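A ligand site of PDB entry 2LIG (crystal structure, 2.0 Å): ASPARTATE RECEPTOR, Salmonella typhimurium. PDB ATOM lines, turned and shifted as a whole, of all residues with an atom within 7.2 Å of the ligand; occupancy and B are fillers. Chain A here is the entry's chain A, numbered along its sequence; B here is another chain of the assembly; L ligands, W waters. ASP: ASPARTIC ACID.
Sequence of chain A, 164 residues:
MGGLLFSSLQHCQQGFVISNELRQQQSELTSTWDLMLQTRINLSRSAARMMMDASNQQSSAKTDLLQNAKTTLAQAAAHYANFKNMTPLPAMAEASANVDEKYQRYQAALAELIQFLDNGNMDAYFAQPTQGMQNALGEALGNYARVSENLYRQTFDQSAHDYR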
ATOM      1  N   ARG A  40       1.695   0.163  -2.855  1.00  0.00           N
ATOM      2  CA  ARG A  40       0.756   0.248  -1.817  1.00  0.00           C
ATOM      3  C   ARG A  40       1.416  -0.014  -0.417  1.00  0.00           C
ATOM      4  O   ARG A  40       1.058   0.687   0.571  1.00  0.00           O
ATOM      5  CB  ARG A  40      -0.416  -0.849  -2.129  1.00  0.00           C
ATOM      6  CG  ARG A  40      -1.569  -0.668  -1.093  1.00  0.00           C
ATOM      7  CD  ARG A  40      -2.839  -1.355  -1.656  1.00  0.00           C
ATOM      8  NE  ARG A  40      -3.932  -1.347  -0.756  1.00  0.00           N
ATOM      9  CZ  ARG A  40      -4.822  -2.272  -0.585  1.00  0.00           C
ATOM     10  NH1 ARG A  40      -4.706  -3.393  -1.327  1.00  0.00           N
ATOM     11  NH2 ARG A  40      -5.859  -2.234   0.250  1.00  0.00           N
ATOM     12  N   ILE A  41       2.382  -0.886  -0.374  1.00  0.00           N
ATOM     13  CA  ILE A  41       3.176  -1.217   0.843  1.00  0.00           C
ATOM     14  C   ILE A  41       3.933   0.034   1.310  1.00  0.00           C
ATOM     15  O   ILE A  41       3.853   0.553   2.410  1.00  0.00           O
ATOM     16  CB  ILE A  41       4.152  -2.374   0.555  1.00  0.00           C
ATOM     17  CG1 ILE A  41       3.539  -3.737   0.381  1.00  0.00           C
ATOM     18  CG2 ILE A  41       5.175  -2.364   1.829  1.00  0.00           C
ATOM     19  CD1 ILE A  41       4.568  -4.778  -0.065  1.00  0.00           C
ATOM     20  N   LEU A  43       3.364   3.043   0.559  1.00  0.00           N
ATOM     21  CA  LEU A  43       2.455   4.111   0.970  1.00  0.00           C
ATOM     22  C   LEU A  43       1.985   3.849   2.423  1.00  0.00           C
ATOM     23  O   LEU A  43       1.841   4.731   3.159  1.00  0.00           O
ATOM     24  CB  LEU A  43       1.208   4.115   0.010  1.00  0.00           C
ATOM     25  CG  LEU A  43       1.338   4.793  -1.368  1.00  0.00           C
ATOM     26  CD1 LEU A  43       0.101   4.610  -2.169  1.00  0.00           C
ATOM     27  CD2 LEU A  43       1.630   6.212  -1.146  1.00  0.00           C
ATOM     28  N   SER A  44       1.861   2.562   2.729  1.00  0.00           N
ATOM     29  CA  SER A  44       1.317   2.221   4.085  1.00  0.00           C
ATOM     30  C   SER A  44       2.497   2.575   5.035  1.00  0.00           C
ATOM     31  O   SER A  44       2.191   3.026   6.183  1.00  0.00           O
ATOM     32  CB  SER A  44       1.013   0.813   4.102  1.00  0.00           C
ATOM     33  OG  SER A  44       0.091   0.615   5.147  1.00  0.00           O
ATOM     34  N   ALA A  47       2.563   6.332   5.735  1.00  0.00           N
ATOM     35  CA  ALA A  47       1.461   6.740   6.555  1.00  0.00           C
ATOM     36  C   ALA A  47       1.662   6.339   8.046  1.00  0.00           C
ATOM     37  O   ALA A  47       1.352   7.154   8.884  1.00  0.00           O
ATOM     38  CB  ALA A  47       0.171   6.056   6.211  1.00  0.00           C
ATOM     39  N   TYR A 106      -6.814   1.144 -11.131  1.00  0.00           N
ATOM     40  CA  TYR A 106      -5.949   0.979  -9.910  1.00  0.00           C
ATOM     41  C   TYR A 106      -4.696   1.898  -9.951  1.00  0.00           C
ATOM     42  O   TYR A 106      -4.234   2.261  -8.908  1.00  0.00           O
ATOM     43  CB  TYR A 106      -5.571  -0.503  -9.807  1.00  0.00           C
ATOM     44  CG  TYR A 106      -4.938  -0.898  -8.494  1.00  0.00           C
ATOM     45  CD1 TYR A 106      -5.259  -0.257  -7.276  1.00  0.00           C
ATOM     46  CD2 TYR A 106      -3.928  -1.837  -8.437  1.00  0.00           C
ATOM     47  CE1 TYR A 106      -4.645  -0.617  -6.078  1.00  0.00           C
ATOM     48  CE2 TYR A 106      -3.259  -2.174  -7.320  1.00  0.00           C
ATOM     49  CZ  TYR A 106      -3.651  -1.541  -6.139  1.00  0.00           C
ATOM     50  OH  TYR A 106      -3.035  -1.911  -4.944  1.00  0.00           O
ATOM     51  N   LEU A 110      -3.791   4.513  -6.836  1.00  0.00           N
ATOM     52  CA  LEU A 110      -2.515   4.658  -6.139  1.00  0.00           C
ATOM     53  C   LEU A 110      -1.954   6.096  -6.315  1.00  0.00           C
ATOM     54  O   LEU A 110      -1.480   6.629  -5.306  1.00  0.00           O
ATOM     55  CB  LEU A 110      -1.553   3.622  -6.629  1.00  0.00           C
ATOM     56  CG  LEU A 110      -1.822   2.164  -6.378  1.00  0.00           C
ATOM     57  CD1 LEU A 110      -0.747   1.340  -7.048  1.00  0.00           C
ATOM     58  CD2 LEU A 110      -1.879   1.911  -4.885  1.00  0.00           C
ATOM     59  N   LEU A 113      -3.727   8.205  -3.821  1.00  0.00           N
ATOM     60  CA  LEU A 113      -3.234   8.068  -2.494  1.00  0.00           C
ATOM     61  C   LEU A 113      -1.910   8.704  -2.262  1.00  0.00           C
ATOM     62  O   LEU A 113      -1.707   9.229  -1.198  1.00  0.00           O
ATOM     63  CB  LEU A 113      -3.118   6.655  -2.080  1.00  0.00           C
ATOM     64  CG  LEU A 113      -4.313   5.746  -1.982  1.00  0.00           C
ATOM     65  CD1 LEU A 113      -3.766   4.405  -1.717  1.00  0.00           C
ATOM     66  CD2 LEU A 113      -5.297   6.167  -0.845  1.00  0.00           C
ATOM     67  N   MET A 122      -4.670  12.449   5.632  1.00  0.00           N
ATOM     68  CA  MET A 122      -4.764  11.109   6.179  1.00  0.00           C
ATOM     69  C   MET A 122      -6.110  10.503   6.060  1.00  0.00           C
ATOM     70  O   MET A 122      -6.219   9.311   5.712  1.00  0.00           O
ATOM     71  CB  MET A 122      -4.343  11.074   7.615  1.00  0.00           C
ATOM     72  CG  MET A 122      -2.971  11.739   7.777  1.00  0.00           C
ATOM     73  SD  MET A 122      -1.652  10.890   6.904  1.00  0.00           S
ATOM     74  CE  MET A 122      -1.305   9.772   8.190  1.00  0.00           C
ATOM     75  N   ALA A 124      -8.459  10.964   3.957  1.00  0.00           N
ATOM     76  CA  ALA A 124      -8.802  10.548   2.613  1.00  0.00           C
ATOM     77  C   ALA A 124      -8.032   9.312   2.138  1.00  0.00           C
ATOM     78  O   ALA A 124      -8.453   8.435   1.367  1.00  0.00           O
ATOM     79  CB  ALA A 124      -8.535  11.680   1.635  1.00  0.00           C
ATOM     80  N   TYR A 125      -6.725   9.243   2.535  1.00  0.00           N
ATOM     81  CA  TYR A 125      -5.846   8.119   2.311  1.00  0.00           C
ATOM     82  C   TYR A 125      -6.531   6.826   2.924  1.00  0.00           C
ATOM     83  O   TYR A 125      -6.734   5.840   2.254  1.00  0.00           O
ATOM     84  CB  TYR A 125      -4.502   8.459   2.892  1.00  0.00           C
ATOM     85  CG  TYR A 125      -3.633   7.246   2.968  1.00  0.00           C
ATOM     86  CD1 TYR A 125      -2.935   6.755   1.826  1.00  0.00           C
ATOM     87  CD2 TYR A 125      -3.517   6.607   4.185  1.00  0.00           C
ATOM     88  CE1 TYR A 125      -2.215   5.649   1.962  1.00  0.00           C
ATOM     89  CE2 TYR A 125      -2.794   5.492   4.319  1.00  0.00           C
ATOM     90  CZ  TYR A 125      -2.096   5.000   3.176  1.00  0.00           C
ATOM     91  OH  TYR A 125      -1.494   3.783   3.300  1.00  0.00           O
ATOM     92  N   PHE A 126      -6.870   6.856   4.231  1.00  0.00           N
ATOM     93  CA  PHE A 126      -7.529   5.696   4.932  1.00  0.00           C
ATOM     94  C   PHE A 126      -8.875   5.366   4.353  1.00  0.00           C
ATOM     95  O   PHE A 126      -9.271   4.173   4.271  1.00  0.00           O
ATOM     96  CB  PHE A 126      -7.658   5.903   6.340  1.00  0.00           C
ATOM     97  CG  PHE A 126      -6.229   5.860   7.048  1.00  0.00           C
ATOM     98  CD1 PHE A 126      -5.606   4.613   7.058  1.00  0.00           C
ATOM     99  CD2 PHE A 126      -5.651   6.988   7.572  1.00  0.00           C
ATOM    100  CE1 PHE A 126      -4.378   4.553   7.636  1.00  0.00           C
ATOM    101  CE2 PHE A 126      -4.422   6.928   8.149  1.00  0.00           C
ATOM    102  CZ  PHE A 126      -3.781   5.739   8.197  1.00  0.00           C
ATOM    103  N   ALA A 127      -9.705   6.359   3.967  1.00  0.00           N
ATOM    104  CA  ALA A 127     -11.098   6.083   3.379  1.00  0.00           C
ATOM    105  C   ALA A 127     -11.117   5.609   2.000  1.00  0.00           C
ATOM    106  O   ALA A 127     -12.163   5.076   1.641  1.00  0.00           O
ATOM    107  CB  ALA A 127     -11.914   7.398   3.497  1.00  0.00           C
ATOM    108  N   GLN A 128     -10.130   5.728   1.081  1.00  0.00           N
ATOM    109  CA  GLN A 128     -10.218   5.252  -0.358  1.00  0.00           C
ATOM    110  C   GLN A 128     -10.376   3.747  -0.397  1.00  0.00           C
ATOM    111  O   GLN A 128      -9.616   3.023   0.285  1.00  0.00           O
ATOM    112  CB  GLN A 128      -8.930   5.612  -1.086  1.00  0.00           C
ATOM    113  CG  GLN A 128      -9.108   5.514  -2.643  1.00  0.00           C
ATOM    114  CD  GLN A 128      -7.826   5.427  -3.334  1.00  0.00           C
ATOM    115  OE1 GLN A 128      -7.225   4.303  -3.287  1.00  0.00           O
ATOM    116  NE2 GLN A 128      -7.357   6.377  -4.023  1.00  0.00           N
ATOM    117  N   PRO A 129     -11.414   3.217  -1.096  1.00  0.00           N
ATOM    118  CA  PRO A 129     -11.589   1.736  -1.252  1.00  0.00           C
ATOM    119  C   PRO A 129     -10.660   1.118  -2.292  1.00  0.00           C
ATOM    120  O   PRO A 129     -11.032   0.628  -3.328  1.00  0.00           O
ATOM    121  CB  PRO A 129     -13.112   1.626  -1.743  1.00  0.00           C
ATOM    122  CG  PRO A 129     -13.286   2.947  -2.480  1.00  0.00           C
ATOM    123  CD  PRO A 129     -12.598   3.937  -1.595  1.00  0.00           C
ATOM    124  N   THR A 130      -9.346   1.210  -1.938  1.00  0.00           N
ATOM    125  CA  THR A 130      -8.241   0.816  -2.763  1.00  0.00           C
ATOM    126  C   THR A 130      -8.319  -0.698  -2.983  1.00  0.00           C
ATOM    127  O   THR A 130      -8.055  -1.175  -4.069  1.00  0.00           O
ATOM    128  CB  THR A 130      -6.917   1.165  -1.947  1.00  0.00           C
ATOM    129  OG1 THR A 130      -7.080   2.434  -1.291  1.00  0.00           O
ATOM    130  CG2 THR A 130      -5.781   1.178  -2.926  1.00  0.00           C
ATOM    131  N   GLN A 131      -8.746  -1.436  -1.959  1.00  0.00           N
ATOM    132  CA  GLN A 131      -8.726  -2.902  -1.977  1.00  0.00           C
ATOM    133  C   GLN A 131      -9.558  -3.421  -3.106  1.00  0.00           C
ATOM    134  O   GLN A 131      -9.228  -4.447  -3.675  1.00  0.00           O
ATOM    135  CB  GLN A 131      -9.190  -3.430  -0.645  1.00  0.00           C
ATOM    136  CG  GLN A 131      -9.055  -4.954  -0.611  1.00  0.00           C
ATOM    137  CD  GLN A 131      -7.644  -5.497  -0.588  1.00  0.00           C
ATOM    138  OE1 GLN A 131      -6.665  -4.878  -0.006  1.00  0.00           O
ATOM    139  NE2 GLN A 131      -7.336  -6.595  -1.188  1.00  0.00           N
ATOM    140  N   ILE B  41       0.837  -6.033   2.954  1.00  0.00           N
ATOM    141  CA  ILE B  41      -0.046  -4.898   2.836  1.00  0.00           C
ATOM    142  C   ILE B  41      -1.130  -5.067   3.898  1.00  0.00           C
ATOM    143  O   ILE B  41      -1.394  -4.130   4.590  1.00  0.00           O
ATOM    144  CB  ILE B  41      -0.805  -4.967   1.472  1.00  0.00           C
ATOM    145  CG1 ILE B  41       0.229  -4.641   0.327  1.00  0.00           C
ATOM    146  CG2 ILE B  41      -1.868  -3.862   1.334  1.00  0.00           C
ATOM    147  CD1 ILE B  41      -0.232  -4.988  -1.067  1.00  0.00           C
ATOM    148  N   SER B  44       0.673  -4.071   7.297  1.00  0.00           N
ATOM    149  CA  SER B  44       0.830  -2.650   7.416  1.00  0.00           C
ATOM    150  C   SER B  44      -0.458  -1.813   7.485  1.00  0.00           C
ATOM    151  O   SER B  44      -0.590  -0.959   8.346  1.00  0.00           O
ATOM    152  CB  SER B  44       1.605  -2.083   6.197  1.00  0.00           C
ATOM    153  OG  SER B  44       2.816  -2.713   5.817  1.00  0.00           O
ATOM    154  N   ARG B  45      -1.492  -2.089   6.667  1.00  0.00           N
ATOM    155  CA  ARG B  45      -2.795  -1.497   6.853  1.00  0.00           C
ATOM    156  C   ARG B  45      -3.323  -1.770   8.248  1.00  0.00           C
ATOM    157  O   ARG B  45      -4.010  -0.907   8.852  1.00  0.00           O
ATOM    158  CB  ARG B  45      -3.764  -1.944   5.891  1.00  0.00           C
ATOM    159  CG  ARG B  45      -3.348  -1.621   4.441  1.00  0.00           C
ATOM    160  CD  ARG B  45      -4.430  -2.102   3.504  1.00  0.00           C
ATOM    161  NE  ARG B  45      -5.635  -1.286   3.735  1.00  0.00           N
ATOM    162  CZ  ARG B  45      -6.862  -1.780   3.629  1.00  0.00           C
ATOM    163  NH1 ARG B  45      -7.082  -3.016   3.302  1.00  0.00           N
ATOM    164  NH2 ARG B  45      -7.818  -1.009   3.998  1.00  0.00           N
ATOM    165  N   SER B  46      -3.089  -2.897   8.865  1.00  0.00           N
ATOM    166  CA  SER B  46      -3.546  -3.155  10.315  1.00  0.00           C
ATOM    167  C   SER B  46      -2.716  -2.366  11.212  1.00  0.00           C
ATOM    168  O   SER B  46      -3.258  -1.708  12.186  1.00  0.00           O
ATOM    169  CB  SER B  46      -3.475  -4.603  10.570  1.00  0.00           C
ATOM    170  OG  SER B  46      -3.859  -4.964  11.911  1.00  0.00           O
ATOM    171  N   ALA B  48      -1.049   0.641  10.927  1.00  0.00           N
ATOM    172  CA  ALA B  48      -1.496   2.021  10.862  1.00  0.00           C
ATOM    173  C   ALA B  48      -2.838   2.180  11.543  1.00  0.00           C
ATOM    174  O   ALA B  48      -2.966   3.130  12.319  1.00  0.00           O
ATOM    175  CB  ALA B  48      -1.705   2.420   9.366  1.00  0.00           C
ATOM    176  N   ARG B  49      -3.824   1.291  11.432  1.00  0.00           N
ATOM    177  CA  ARG B  49      -5.060   1.324  12.131  1.00  0.00           C
ATOM    178  C   ARG B  49      -4.936   1.122  13.641  1.00  0.00           C
ATOM    179  O   ARG B  49      -5.747   1.687  14.380  1.00  0.00           O
ATOM    180  CB  ARG B  49      -6.038   0.259  11.593  1.00  0.00           C
ATOM    181  CG  ARG B  49      -6.637   0.781  10.358  1.00  0.00           C
ATOM    182  CD  ARG B  49      -7.529  -0.199   9.569  1.00  0.00           C
ATOM    183  NE  ARG B  49      -8.195   0.503   8.479  1.00  0.00           N
ATOM    184  CZ  ARG B  49      -7.550   0.883   7.323  1.00  0.00           C
ATOM    185  NH1 ARG B  49      -6.258   0.679   7.063  1.00  0.00           N
ATOM    186  NH2 ARG B  49      -8.204   1.483   6.314  1.00  0.00           N
ATOM    187  N   MET B  52      -4.498   4.559  15.392  1.00  0.00           N
ATOM    188  CA  MET B  52      -5.587   5.489  15.291  1.00  0.00           C
ATOM    189  C   MET B  52      -6.509   5.466  16.524  1.00  0.00           C
ATOM    190  O   MET B  52      -6.121   4.945  17.502  1.00  0.00           O
ATOM    191  CB  MET B  52      -6.514   5.111  14.143  1.00  0.00           C
ATOM    192  CG  MET B  52      -6.130   5.472  12.802  1.00  0.00           C
ATOM    193  SD  MET B  52      -7.438   4.463  11.962  1.00  0.00           S
ATOM    194  CE  MET B  52      -6.645   4.408  10.364  1.00  0.00           C
ATOM    195  N   LEU B  65      -8.240  -7.271   8.782  1.00  0.00           N
ATOM    196  CA  LEU B  65      -6.987  -7.145   8.059  1.00  0.00           C
ATOM    197  C   LEU B  65      -6.002  -8.160   8.644  1.00  0.00           C
ATOM    198  O   LEU B  65      -5.386  -8.832   7.843  1.00  0.00           O
ATOM    199  CB  LEU B  65      -6.439  -5.787   8.186  1.00  0.00           C
ATOM    200  CG  LEU B  65      -6.642  -4.674   7.111  1.00  0.00           C
ATOM    201  CD1 LEU B  65      -7.547  -5.198   5.930  1.00  0.00           C
ATOM    202  CD2 LEU B  65      -7.015  -3.406   7.855  1.00  0.00           C
HETATM  203  N   ASP L   1      -6.840   3.116   1.504  1.00  0.00           N
HETATM  204  CA  ASP L   1      -5.432   2.851   1.642  1.00  0.00           C
HETATM  205  C   ASP L   1      -5.135   1.405   1.231  1.00  0.00           C
HETATM  206  O   ASP L   1      -3.982   1.191   0.873  1.00  0.00           O
HETATM  207  CB  ASP L   1      -4.858   2.964   2.899  1.00  0.00           C
HETATM  208  CG  ASP L   1      -5.388   2.173   4.073  1.00  0.00           C
HETATM  209  OD1 ASP L   1      -6.605   1.845   4.160  1.00  0.00           O
HETATM  210  OD2 ASP L   1      -4.695   1.887   5.012  1.00  0.00           O
HETATM  211  OXT ASP L   1      -6.049   0.588   1.201  1.00  0.00           O
HETATM  212  O   HOH W   1      -8.772   0.043   0.646  1.00  0.00           O
HETATM  213  O   HOH W   2      -1.373   2.171   1.060  1.00  0.00           O
HETATM  214  O   HOH W   3      -9.684   2.042   2.628  1.00  0.00           O
HETATM  215  O   HOH W   4      -1.986   2.095   5.414  1.00  0.00           O
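Phe 126 touches the ligand. Hydrophobic or aromatic side chains within 4 Å of the ligand: Tyr 125 and Phe 126. Seven residues have an atom within 4 Å of the ligand: Arg 40, Tyr 125, Phe 126, Gln 128, Thr 130, Arg 45 of chain B and Arg 49 of chain B.
The side-chain amide oxygen (OE1) of Gln 131 is in hydrogen-bond range of the guanidinium group (NH2) of Arg 40, at 2.8 Å. The backbone NH (N) of Arg 45 of chain B sits at hydrogen-bond distance from the side-chain hydroxyl (OG) of Ser 44 of chain A, at 3.5 Å. OG1 of Thr 130 lies within hydrogen-bond range of OE1 of Gln 128 (2.7 Å). The guanidinium group (NH1) of Arg 49 of chain B sits at hydrogen-bond distance from the backbone carbonyl oxygen (O) of Arg 45 of chain B. The backbone carbonyl oxygen of Leu 43 is in hydrogen-bond range of the side-chain hydroxyl of Tyr 125 (3.5 Å).
Water W4 lies within hydrogen-bond range of the side-chain hydroxyl (OG) of Ser 44 of chain A (2.6 Å), an oxygen (OD2) of the ligand (2.7 Å) and the side-chain hydroxyl (OH) of Tyr 125 (2.7 Å). Water W2 lies within hydrogen-bond range of OH of Tyr 125 (2.8 Å), O of the ligand (2.8 Å) and O of Arg 40 (2.9 Å). Water W1 lies within hydrogen-bond range of an oxygen (OXT) of the ligand (2.8 Å), the backbone NH of Thr 130 (2.9 Å), the backbone NH of Gln 131 (3.0 Å) and the backbone carbonyl oxygen of Gln 128 (3.1 Å). Water W3 lies within hydrogen-bond range of O of Gln 128, O of Phe 126 and N of the ligand.
NH2 of Arg 40 lies within salt-bridge range of OXT of the ligand. O of Gln 128 is in hydrogen-bond range of N of the ligand, at 3.0 Å. A nitrogen (N) of the ligand lies within hydrogen-bond range of the side-chain hydroxyl of Thr 130 (2.9 Å). The guanidinium group (NH2) of Arg 45 of chain B is in salt-bridge range of an oxygen (OD1) of the ligand, 3.1 Å away. The guanidinium group (NH2) of Arg 49 of chain B is in salt-bridge range of an oxygen (OD1) of the ligand, 2.7 Å away. The backbone carbonyl oxygen (O) of Tyr 125 sits at hydrogen-bond distance from a nitrogen (N) of the ligand.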
